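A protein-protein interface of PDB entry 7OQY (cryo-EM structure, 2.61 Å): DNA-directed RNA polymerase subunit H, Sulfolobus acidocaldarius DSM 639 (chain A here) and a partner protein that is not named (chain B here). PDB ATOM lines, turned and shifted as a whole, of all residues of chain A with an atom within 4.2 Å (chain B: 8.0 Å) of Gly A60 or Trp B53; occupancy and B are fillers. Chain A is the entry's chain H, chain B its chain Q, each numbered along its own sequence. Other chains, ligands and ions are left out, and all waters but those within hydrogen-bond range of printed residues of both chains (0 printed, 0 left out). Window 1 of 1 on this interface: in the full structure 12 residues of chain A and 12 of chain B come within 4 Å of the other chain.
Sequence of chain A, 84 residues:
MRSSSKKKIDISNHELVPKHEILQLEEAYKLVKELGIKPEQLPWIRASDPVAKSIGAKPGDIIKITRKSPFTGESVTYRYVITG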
ATOM      1  N   LEU A  25      10.945   0.133  -5.303  1.00  0.00           N
ATOM      2  CA  LEU A  25      11.586  -1.103  -4.861  1.00  0.00           C
ATOM      3  C   LEU A  25      12.623  -1.595  -5.864  1.00  0.00           C
ATOM      4  O   LEU A  25      13.676  -2.103  -5.469  1.00  0.00           O
ATOM      5  CB  LEU A  25      10.541  -2.185  -4.601  1.00  0.00           C
ATOM      6  CG  LEU A  25      11.108  -3.390  -3.846  1.00  0.00           C
ATOM      7  CD1 LEU A  25      11.874  -2.934  -2.614  1.00  0.00           C
ATOM      8  CD2 LEU A  25      10.019  -4.368  -3.462  1.00  0.00           C
ATOM      9  N   TYR A  29      16.500  -1.967  -4.925  1.00  0.00           N
ATOM     10  CA  TYR A  29      17.154  -3.255  -5.126  1.00  0.00           C
ATOM     11  C   TYR A  29      18.410  -3.099  -5.972  1.00  0.00           C
ATOM     12  O   TYR A  29      19.470  -3.643  -5.638  1.00  0.00           O
ATOM     13  CB  TYR A  29      16.170  -4.231  -5.776  1.00  0.00           C
ATOM     14  CG  TYR A  29      16.781  -5.529  -6.252  1.00  0.00           C
ATOM     15  CD1 TYR A  29      16.906  -6.615  -5.396  1.00  0.00           C
ATOM     16  CD2 TYR A  29      17.218  -5.676  -7.562  1.00  0.00           C
ATOM     17  CE1 TYR A  29      17.458  -7.803  -5.829  1.00  0.00           C
ATOM     18  CE2 TYR A  29      17.773  -6.859  -8.001  1.00  0.00           C
ATOM     19  CZ  TYR A  29      17.889  -7.919  -7.131  1.00  0.00           C
ATOM     20  OH  TYR A  29      18.441  -9.101  -7.568  1.00  0.00           O
ATOM     21  N   VAL A  32      21.159  -1.401  -3.804  1.00  0.00           N
ATOM     22  CA  VAL A  32      21.809  -2.257  -2.816  1.00  0.00           C
ATOM     23  C   VAL A  32      22.641  -3.343  -3.491  1.00  0.00           C
ATOM     24  O   VAL A  32      23.645  -3.794  -2.930  1.00  0.00           O
ATOM     25  CB  VAL A  32      20.783  -2.855  -1.833  1.00  0.00           C
ATOM     26  CG1 VAL A  32      20.003  -1.749  -1.145  1.00  0.00           C
ATOM     27  CG2 VAL A  32      19.848  -3.820  -2.535  1.00  0.00           C
ATOM     28  N   PRO A  39      20.592  -3.589   3.207  1.00  0.00           N
ATOM     29  CA  PRO A  39      19.929  -2.283   3.359  1.00  0.00           C
ATOM     30  C   PRO A  39      20.244  -1.578   4.667  1.00  0.00           C
ATOM     31  O   PRO A  39      20.281  -0.342   4.693  1.00  0.00           O
ATOM     32  CB  PRO A  39      18.441  -2.635   3.251  1.00  0.00           C
ATOM     33  CG  PRO A  39      18.411  -3.910   2.492  1.00  0.00           C
ATOM     34  CD  PRO A  39      19.628  -4.664   2.917  1.00  0.00           C
ATOM     35  N   LYS A  58       7.489   4.193   5.298  1.00  0.00           N
ATOM     36  CA  LYS A  58       7.347   3.055   6.186  1.00  0.00           C
ATOM     37  C   LYS A  58       8.672   2.320   6.335  1.00  0.00           C
ATOM     38  O   LYS A  58       9.525   2.369   5.443  1.00  0.00           O
ATOM     39  CB  LYS A  58       6.275   2.092   5.660  1.00  0.00           C
ATOM     40  CG  LYS A  58       4.862   2.643   5.742  1.00  0.00           C
ATOM     41  CD  LYS A  58       4.468   2.921   7.185  1.00  0.00           C
ATOM     42  CE  LYS A  58       3.119   3.617   7.268  1.00  0.00           C
ATOM     43  NZ  LYS A  58       3.188   5.026   6.789  1.00  0.00           N
ATOM     44  N   PRO A  59       8.883   1.639   7.461  1.00  0.00           N
ATOM     45  CA  PRO A  59      10.140   0.905   7.657  1.00  0.00           C
ATOM     46  C   PRO A  59      10.363  -0.140   6.575  1.00  0.00           C
ATOM     47  O   PRO A  59       9.430  -0.802   6.117  1.00  0.00           O
ATOM     48  CB  PRO A  59       9.961   0.264   9.035  1.00  0.00           C
ATOM     49  CG  PRO A  59       9.004   1.167   9.734  1.00  0.00           C
ATOM     50  CD  PRO A  59       8.058   1.652   8.680  1.00  0.00           C
ATOM     51  N   GLY A  60      11.625  -0.285   6.175  1.00  0.00           N
ATOM     52  CA  GLY A  60      12.001  -1.112   5.052  1.00  0.00           C
ATOM     53  C   GLY A  60      12.181  -0.353   3.757  1.00  0.00           C
ATOM     54  O   GLY A  60      12.668  -0.933   2.780  1.00  0.00           O
ATOM     55  N   ASP A  61      11.803   0.920   3.723  1.00  0.00           N
ATOM     56  CA  ASP A  61      11.985   1.768   2.557  1.00  0.00           C
ATOM     57  C   ASP A  61      13.373   2.398   2.568  1.00  0.00           C
ATOM     58  O   ASP A  61      14.085   2.388   3.573  1.00  0.00           O
ATOM     59  CB  ASP A  61      10.915   2.861   2.517  1.00  0.00           C
ATOM     60  CG  ASP A  61       9.583   2.359   2.006  1.00  0.00           C
ATOM     61  OD1 ASP A  61       9.573   1.394   1.215  1.00  0.00           O
ATOM     62  OD2 ASP A  61       8.542   2.926   2.399  1.00  0.00           O
ATOM     63  N   TYR A  80      17.980   4.572   5.215  1.00  0.00           N
ATOM     64  CA  TYR A  80      17.151   3.389   5.394  1.00  0.00           C
ATOM     65  C   TYR A  80      16.200   3.612   6.561  1.00  0.00           C
ATOM     66  O   TYR A  80      16.633   3.991   7.654  1.00  0.00           O
ATOM     67  CB  TYR A  80      18.019   2.153   5.636  1.00  0.00           C
ATOM     68  CG  TYR A  80      17.240   0.886   5.886  1.00  0.00           C
ATOM     69  CD1 TYR A  80      16.578   0.242   4.853  1.00  0.00           C
ATOM     70  CD2 TYR A  80      17.174   0.330   7.154  1.00  0.00           C
ATOM     71  CE1 TYR A  80      15.867  -0.915   5.077  1.00  0.00           C
ATOM     72  CE2 TYR A  80      16.463  -0.824   7.387  1.00  0.00           C
ATOM     73  CZ  TYR A  80      15.813  -1.443   6.346  1.00  0.00           C
ATOM     74  OH  TYR A  80      15.106  -2.598   6.574  1.00  0.00           O
ATOM     75  N   VAL A  81      14.912   3.372   6.330  1.00  0.00           N
ATOM     76  CA  VAL A  81      13.879   3.664   7.321  1.00  0.00           C
ATOM     77  C   VAL A  81      13.836   2.539   8.347  1.00  0.00           C
ATOM     78  O   VAL A  81      13.651   1.370   7.995  1.00  0.00           O
ATOM     79  CB  VAL A  81      12.510   3.853   6.654  1.00  0.00           C
ATOM     80  CG1 VAL A  81      11.496   4.370   7.659  1.00  0.00           C
ATOM     81  CG2 VAL A  81      12.619   4.797   5.471  1.00  0.00           C
ATOM     82  N   MET B  45       8.521  -5.869  13.712  1.00  0.00           N
ATOM     83  CA  MET B  45       8.409  -5.330  12.360  1.00  0.00           C
ATOM     84  C   MET B  45       9.782  -5.096  11.735  1.00  0.00           C
ATOM     85  O   MET B  45       9.962  -5.310  10.529  1.00  0.00           O
ATOM     86  CB  MET B  45       7.555  -4.062  12.393  1.00  0.00           C
ATOM     87  CG  MET B  45       7.301  -3.394  11.058  1.00  0.00           C
ATOM     88  SD  MET B  45       6.245  -1.946  11.274  1.00  0.00           S
ATOM     89  CE  MET B  45       7.337  -0.796  12.087  1.00  0.00           C
ATOM     90  N   LEU B  46      10.768  -4.680  12.535  1.00  0.00           N
ATOM     91  CA  LEU B  46      12.137  -4.601  12.031  1.00  0.00           C
ATOM     92  C   LEU B  46      12.638  -5.971  11.591  1.00  0.00           C
ATOM     93  O   LEU B  46      13.247  -6.107  10.521  1.00  0.00           O
ATOM     94  CB  LEU B  46      13.056  -4.010  13.103  1.00  0.00           C
ATOM     95  CG  LEU B  46      14.356  -3.336  12.656  1.00  0.00           C
ATOM     96  CD1 LEU B  46      14.091  -2.199  11.691  1.00  0.00           C
ATOM     97  CD2 LEU B  46      15.119  -2.828  13.864  1.00  0.00           C
ATOM     98  N   LEU B  47      12.375  -7.002  12.399  1.00  0.00           N
ATOM     99  CA  LEU B  47      12.782  -8.356  12.033  1.00  0.00           C
ATOM    100  C   LEU B  47      12.102  -8.815  10.748  1.00  0.00           C
ATOM    101  O   LEU B  47      12.743  -9.419   9.881  1.00  0.00           O
ATOM    102  CB  LEU B  47      12.475  -9.321  13.177  1.00  0.00           C
ATOM    103  CG  LEU B  47      12.541 -10.821  12.871  1.00  0.00           C
ATOM    104  CD1 LEU B  47      13.932 -11.228  12.411  1.00  0.00           C
ATOM    105  CD2 LEU B  47      12.124 -11.634  14.082  1.00  0.00           C
ATOM    106  N   LYS B  48      10.801  -8.545  10.611  1.00  0.00           N
ATOM    107  CA  LYS B  48      10.085  -8.954   9.405  1.00  0.00           C
ATOM    108  C   LYS B  48      10.617  -8.238   8.171  1.00  0.00           C
ATOM    109  O   LYS B  48      10.764  -8.851   7.105  1.00  0.00           O
ATOM    110  CB  LYS B  48       8.586  -8.713   9.568  1.00  0.00           C
ATOM    111  CG  LYS B  48       7.936  -9.603  10.610  1.00  0.00           C
ATOM    112  CD  LYS B  48       6.442  -9.362  10.694  1.00  0.00           C
ATOM    113  CE  LYS B  48       5.818 -10.200  11.792  1.00  0.00           C
ATOM    114  NZ  LYS B  48       5.872 -11.651  11.465  1.00  0.00           N
ATOM    115  N   ASP B  49      10.907  -6.940   8.287  1.00  0.00           N
ATOM    116  CA  ASP B  49      11.508  -6.224   7.166  1.00  0.00           C
ATOM    117  C   ASP B  49      12.857  -6.825   6.795  1.00  0.00           C
ATOM    118  O   ASP B  49      13.176  -6.975   5.607  1.00  0.00           O
ATOM    119  CB  ASP B  49      11.654  -4.741   7.505  1.00  0.00           C
ATOM    120  CG  ASP B  49      10.322  -4.032   7.597  1.00  0.00           C
ATOM    121  OD1 ASP B  49       9.374  -4.460   6.906  1.00  0.00           O
ATOM    122  OD2 ASP B  49      10.219  -3.052   8.363  1.00  0.00           O
ATOM    123  N   THR B  50      13.660  -7.181   7.801  1.00  0.00           N
ATOM    124  CA  THR B  50      14.950  -7.807   7.529  1.00  0.00           C
ATOM    125  C   THR B  50      14.781  -9.128   6.785  1.00  0.00           C
ATOM    126  O   THR B  50      15.501  -9.398   5.816  1.00  0.00           O
ATOM    127  CB  THR B  50      15.713  -8.021   8.837  1.00  0.00           C
ATOM    128  OG1 THR B  50      15.968  -6.753   9.454  1.00  0.00           O
ATOM    129  CG2 THR B  50      17.035  -8.723   8.579  1.00  0.00           C
ATOM    130  N   GLU B  51      13.828  -9.959   7.219  1.00  0.00           N
ATOM    131  CA  GLU B  51      13.605 -11.241   6.549  1.00  0.00           C
ATOM    132  C   GLU B  51      13.128 -11.049   5.114  1.00  0.00           C
ATOM    133  O   GLU B  51      13.568 -11.766   4.206  1.00  0.00           O
ATOM    134  CB  GLU B  51      12.604 -12.094   7.328  1.00  0.00           C
ATOM    135  CG  GLU B  51      12.900 -12.233   8.805  1.00  0.00           C
ATOM    136  CD  GLU B  51      11.855 -13.059   9.527  1.00  0.00           C
ATOM    137  OE1 GLU B  51      10.669 -12.984   9.145  1.00  0.00           O
ATOM    138  OE2 GLU B  51      12.220 -13.781  10.480  1.00  0.00           O
ATOM    139  N   ILE B  52      12.216 -10.100   4.889  1.00  0.00           N
ATOM    140  CA  ILE B  52      11.731  -9.860   3.532  1.00  0.00           C
ATOM    141  C   ILE B  52      12.868  -9.389   2.633  1.00  0.00           C
ATOM    142  O   ILE B  52      12.998  -9.841   1.488  1.00  0.00           O
ATOM    143  CB  ILE B  52      10.560  -8.859   3.537  1.00  0.00           C
ATOM    144  CG1 ILE B  52       9.403  -9.392   4.380  1.00  0.00           C
ATOM    145  CG2 ILE B  52      10.086  -8.583   2.119  1.00  0.00           C
ATOM    146  CD1 ILE B  52       8.290  -8.392   4.581  1.00  0.00           C
ATOM    147  N   TRP B  53      13.710  -8.479   3.132  1.00  0.00           N
ATOM    148  CA  TRP B  53      14.836  -8.008   2.330  1.00  0.00           C
ATOM    149  C   TRP B  53      15.820  -9.135   2.038  1.00  0.00           C
ATOM    150  O   TRP B  53      16.340  -9.239   0.920  1.00  0.00           O
ATOM    151  CB  TRP B  53      15.539  -6.849   3.033  1.00  0.00           C
ATOM    152  CG  TRP B  53      15.178  -5.500   2.487  1.00  0.00           C
ATOM    153  CD1 TRP B  53      14.547  -4.492   3.151  1.00  0.00           C
ATOM    154  CD2 TRP B  53      15.430  -5.011   1.163  1.00  0.00           C
ATOM    155  NE1 TRP B  53      14.389  -3.406   2.326  1.00  0.00           N
ATOM    156  CE2 TRP B  53      14.924  -3.699   1.099  1.00  0.00           C
ATOM    157  CE3 TRP B  53      16.037  -5.555   0.026  1.00  0.00           C
ATOM    158  CZ2 TRP B  53      15.002  -2.924  -0.055  1.00  0.00           C
ATOM    159  CZ3 TRP B  53      16.113  -4.782  -1.119  1.00  0.00           C
ATOM    160  CH2 TRP B  53      15.599  -3.483  -1.150  1.00  0.00           C
ATOM    161  N   ASP B  54      16.093  -9.987   3.031  1.00  0.00           N
ATOM    162  CA  ASP B  54      16.995 -11.115   2.814  1.00  0.00           C
ATOM    163  C   ASP B  54      16.452 -12.054   1.745  1.00  0.00           C
ATOM    164  O   ASP B  54      17.188 -12.488   0.850  1.00  0.00           O
ATOM    165  CB  ASP B  54      17.216 -11.873   4.122  1.00  0.00           C
ATOM    166  CG  ASP B  54      18.050 -11.094   5.116  1.00  0.00           C
ATOM    167  OD1 ASP B  54      18.888 -10.276   4.683  1.00  0.00           O
ATOM    168  OD2 ASP B  54      17.871 -11.305   6.334  1.00  0.00           O
ATOM    169  N   LYS B  55      15.161 -12.385   1.825  1.00  0.00           N
ATOM    170  CA  LYS B  55      14.572 -13.292   0.845  1.00  0.00           C
ATOM    171  C   LYS B  55      14.546 -12.670  -0.548  1.00  0.00           C
ATOM    172  O   LYS B  55      14.768 -13.365  -1.546  1.00  0.00           O
ATOM    173  CB  LYS B  55      13.166 -13.699   1.285  1.00  0.00           C
ATOM    174  CG  LYS B  55      13.137 -14.554   2.540  1.00  0.00           C
ATOM    175  CD  LYS B  55      11.736 -15.062   2.836  1.00  0.00           C
ATOM    176  CE  LYS B  55      10.848 -13.952   3.371  1.00  0.00           C
ATOM    177  NZ  LYS B  55       9.506 -14.459   3.769  1.00  0.00           N
ATOM    178  N   LEU B  56      14.270 -11.367  -0.638  1.00  0.00           N
ATOM    179  CA  LEU B  56      14.267 -10.703  -1.938  1.00  0.00           C
ATOM    180  C   LEU B  56      15.664 -10.656  -2.544  1.00  0.00           C
ATOM    181  O   LEU B  56      15.827 -10.834  -3.756  1.00  0.00           O
ATOM    182  CB  LEU B  56      13.690  -9.293  -1.805  1.00  0.00           C
ATOM    183  CG  LEU B  56      13.896  -8.331  -2.976  1.00  0.00           C
ATOM    184  CD1 LEU B  56      13.163  -8.820  -4.215  1.00  0.00           C
ATOM    185  CD2 LEU B  56      13.446  -6.929  -2.602  1.00  0.00           C
ATOM    186  N   LEU B  57      16.686 -10.421  -1.717  1.00  0.00           N
ATOM    187  CA  LEU B  57      18.046 -10.299  -2.228  1.00  0.00           C
ATOM    188  C   LEU B  57      18.618 -11.631  -2.698  1.00  0.00           C
ATOM    189  O   LEU B  57      19.591 -11.637  -3.459  1.00  0.00           O
ATOM    190  CB  LEU B  57      18.955  -9.691  -1.159  1.00  0.00           C
ATOM    191  CG  LEU B  57      18.906  -8.169  -1.024  1.00  0.00           C
ATOM    192  CD1 LEU B  57      19.742  -7.703   0.155  1.00  0.00           C
ATOM    193  CD2 LEU B  57      19.371  -7.504  -2.309  1.00  0.00           C
ATOM    194  N   ARG B  58      18.043 -12.751  -2.267  1.00  0.00           N
ATOM    195  CA  ARG B  58      18.486 -14.074  -2.682  1.00  0.00           C
ATOM    196  C   ARG B  58      17.741 -14.586  -3.908  1.00  0.00           C
ATOM    197  O   ARG B  58      17.913 -15.752  -4.278  1.00  0.00           O
ATOM    198  CB  ARG B  58      18.334 -15.069  -1.530  1.00  0.00           C
ATOM    199  CG  ARG B  58      19.289 -14.829  -0.376  1.00  0.00           C
ATOM    200  CD  ARG B  58      19.389 -16.049   0.522  1.00  0.00           C
ATOM    201  NE  ARG B  58      18.076 -16.563   0.890  1.00  0.00           N
ATOM    202  CZ  ARG B  58      17.524 -16.421   2.087  1.00  0.00           C
ATOM    203  NH1 ARG B  58      18.146 -15.784   3.064  1.00  0.00           N
ATOM    204  NH2 ARG B  58      16.317 -16.933   2.310  1.00  0.00           N
ATOM    205  N   ASN B  59      16.909 -13.747  -4.527  1.00  0.00           N
ATOM    206  CA  ASN B  59      16.121 -14.109  -5.707  1.00  0.00           C
ATOM    207  C   ASN B  59      15.128 -15.228  -5.408  1.00  0.00           C
ATOM    208  O   ASN B  59      14.760 -16.000  -6.297  1.00  0.00           O
ATOM    209  CB  ASN B  59      17.018 -14.486  -6.889  1.00  0.00           C
ATOM    210  CG  ASN B  59      17.857 -13.324  -7.376  1.00  0.00           C
ATOM    211  OD1 ASN B  59      17.345 -12.384  -7.984  1.00  0.00           O
ATOM    212  ND2 ASN B  59      19.157 -13.381  -7.112  1.00  0.00           N
ATOM    213  N   LEU B  61      12.193 -14.263  -4.115  1.00  0.00           N
ATOM    214  CA  LEU B  61      10.959 -13.515  -4.295  1.00  0.00           C
ATOM    215  C   LEU B  61      11.109 -12.567  -5.473  1.00  0.00           C
ATOM    216  O   LEU B  61      12.220 -12.219  -5.883  1.00  0.00           O
ATOM    217  CB  LEU B  61      10.579 -12.709  -3.043  1.00  0.00           C
ATOM    218  CG  LEU B  61       9.813 -13.374  -1.899  1.00  0.00           C
ATOM    219  CD1 LEU B  61      10.665 -14.370  -1.143  1.00  0.00           C
ATOM    220  CD2 LEU B  61       9.298 -12.301  -0.960  1.00  0.00           C
ATOM    221  N   ALA B  66       7.509  -8.925  -2.886  1.00  0.00           N
ATOM    222  CA  ALA B  66       8.154  -8.161  -1.825  1.00  0.00           C
ATOM    223  C   ALA B  66       7.368  -6.898  -1.502  1.00  0.00           C
ATOM    224  O   ALA B  66       7.208  -6.543  -0.329  1.00  0.00           O
ATOM    225  CB  ALA B  66       9.589  -7.818  -2.224  1.00  0.00           C
ATOM    226  N   MET B  69       4.289  -7.955   0.536  1.00  0.00           N
ATOM    227  CA  MET B  69       4.616  -8.318   1.912  1.00  0.00           C
ATOM    228  C   MET B  69       5.006  -7.095   2.738  1.00  0.00           C
ATOM    229  O   MET B  69       4.638  -6.993   3.915  1.00  0.00           O
ATOM    230  CB  MET B  69       5.725  -9.366   1.936  1.00  0.00           C
ATOM    231  CG  MET B  69       5.311 -10.707   1.360  1.00  0.00           C
ATOM    232  SD  MET B  69       6.658 -11.900   1.327  1.00  0.00           S
ATOM    233  CE  MET B  69       6.843 -12.243   3.075  1.00  0.00           C
ATOM    234  N   PHE B  70       5.754  -6.160   2.142  1.00  0.00           N
ATOM    235  CA  PHE B  70       6.090  -4.926   2.846  1.00  0.00           C
ATOM    236  C   PHE B  70       4.833  -4.149   3.212  1.00  0.00           C
ATOM    237  O   PHE B  70       4.701  -3.660   4.341  1.00  0.00           O
ATOM    238  CB  PHE B  70       7.015  -4.063   1.986  1.00  0.00           C
ATOM    239  CG  PHE B  70       8.469  -4.438   2.082  1.00  0.00           C
ATOM    240  CD1 PHE B  70       9.080  -4.596   3.315  1.00  0.00           C
ATOM    241  CD2 PHE B  70       9.228  -4.616   0.937  1.00  0.00           C
ATOM    242  CE1 PHE B  70      10.417  -4.935   3.401  1.00  0.00           C
ATOM    243  CE2 PHE B  70      10.564  -4.956   1.019  1.00  0.00           C
ATOM    244  CZ  PHE B  70      11.158  -5.116   2.252  1.00  0.00           C
ATOM    245  N   ALA B  74       3.543  -3.345   7.016  1.00  0.00           N
ATOM    246  CA  ALA B  74       3.348  -1.953   7.412  1.00  0.00           C
ATOM    247  C   ALA B  74       1.924  -1.704   7.887  1.00  0.00           C
ATOM    248  O   ALA B  74       1.707  -1.007   8.885  1.00  0.00           O
ATOM    249  CB  ALA B  74       3.698  -1.024   6.250  1.00  0.00           C
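Of the 10 printed residues of chain A, 8 touch a printed residue of chain B. Hydrophobic or aromatic side chains of chain A that line the printed part of chain B: Leu A25, Tyr A29, Val A32, Pro A39, Pro A59 and Tyr A80. Printed residues of chain B that touch a printed residue of chain A: Met B45, Asp B49, Trp B53, Leu B57, Asn B59, Ala B66 and Ala B74. Among the printed residues, 10 pairs touch across the chains.
Among the printed residues, pairs that only touch across the chains: Leu A25 with Ala B66 (3.7 Å), Val A32 with Leu B57 (3.7 Å), Pro A39 with Trp B53 (3.4 Å), Lys A58 with Ala B74 (3.9 Å), Pro A59 with Met B45 (3.5 Å), Gly A60 with Asp B49 (3.8 Å) and Tyr A80 with Trp B53 (3.95 Å).
Of chain B, only Asp B49 (3.8 Å) and Trp B53 (3.0 Å) come within 4 Å of Gly A60. Trp B53 touches just these residues of chain A: Pro A39 (3.4 Å), Gly A60 (3.0 Å) and Tyr A80 (3.95 Å). Printed residues of chain A within 4 Å of Leu B57: Val A32. Printed residues of chain B within 4 Å of Pro A39: Trp B53. Asp A61 touches none of the printed residues of chain B. Phe B70 touches none of the printed residues of chain A. The nearest printed residue of chain B that does not touch Pro A39 is Leu B57 (4.1 Å).
The indole nitrogen (NE1) of Trp B53 lies within hydrogen-bond range of the backbone carbonyl oxygen (O) of Gly A60. OH of Tyr A29 lies within hydrogen-bond range of OD1 of Asn B59, at 3.5 Å. The backbone carbonyl oxygen (O) of Pro A59 sits close to the side-chain carboxylate (OD2) of Asp B49 (3.3 Å).
OD2 of Asp A61 lies within hydrogen-bond range of N of Lys A58 (3.3 Å). The backbone NH (N) of Gly A60 sits at hydrogen-bond distance from the backbone carbonyl oxygen (O) of Val A81 (3.2 Å).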
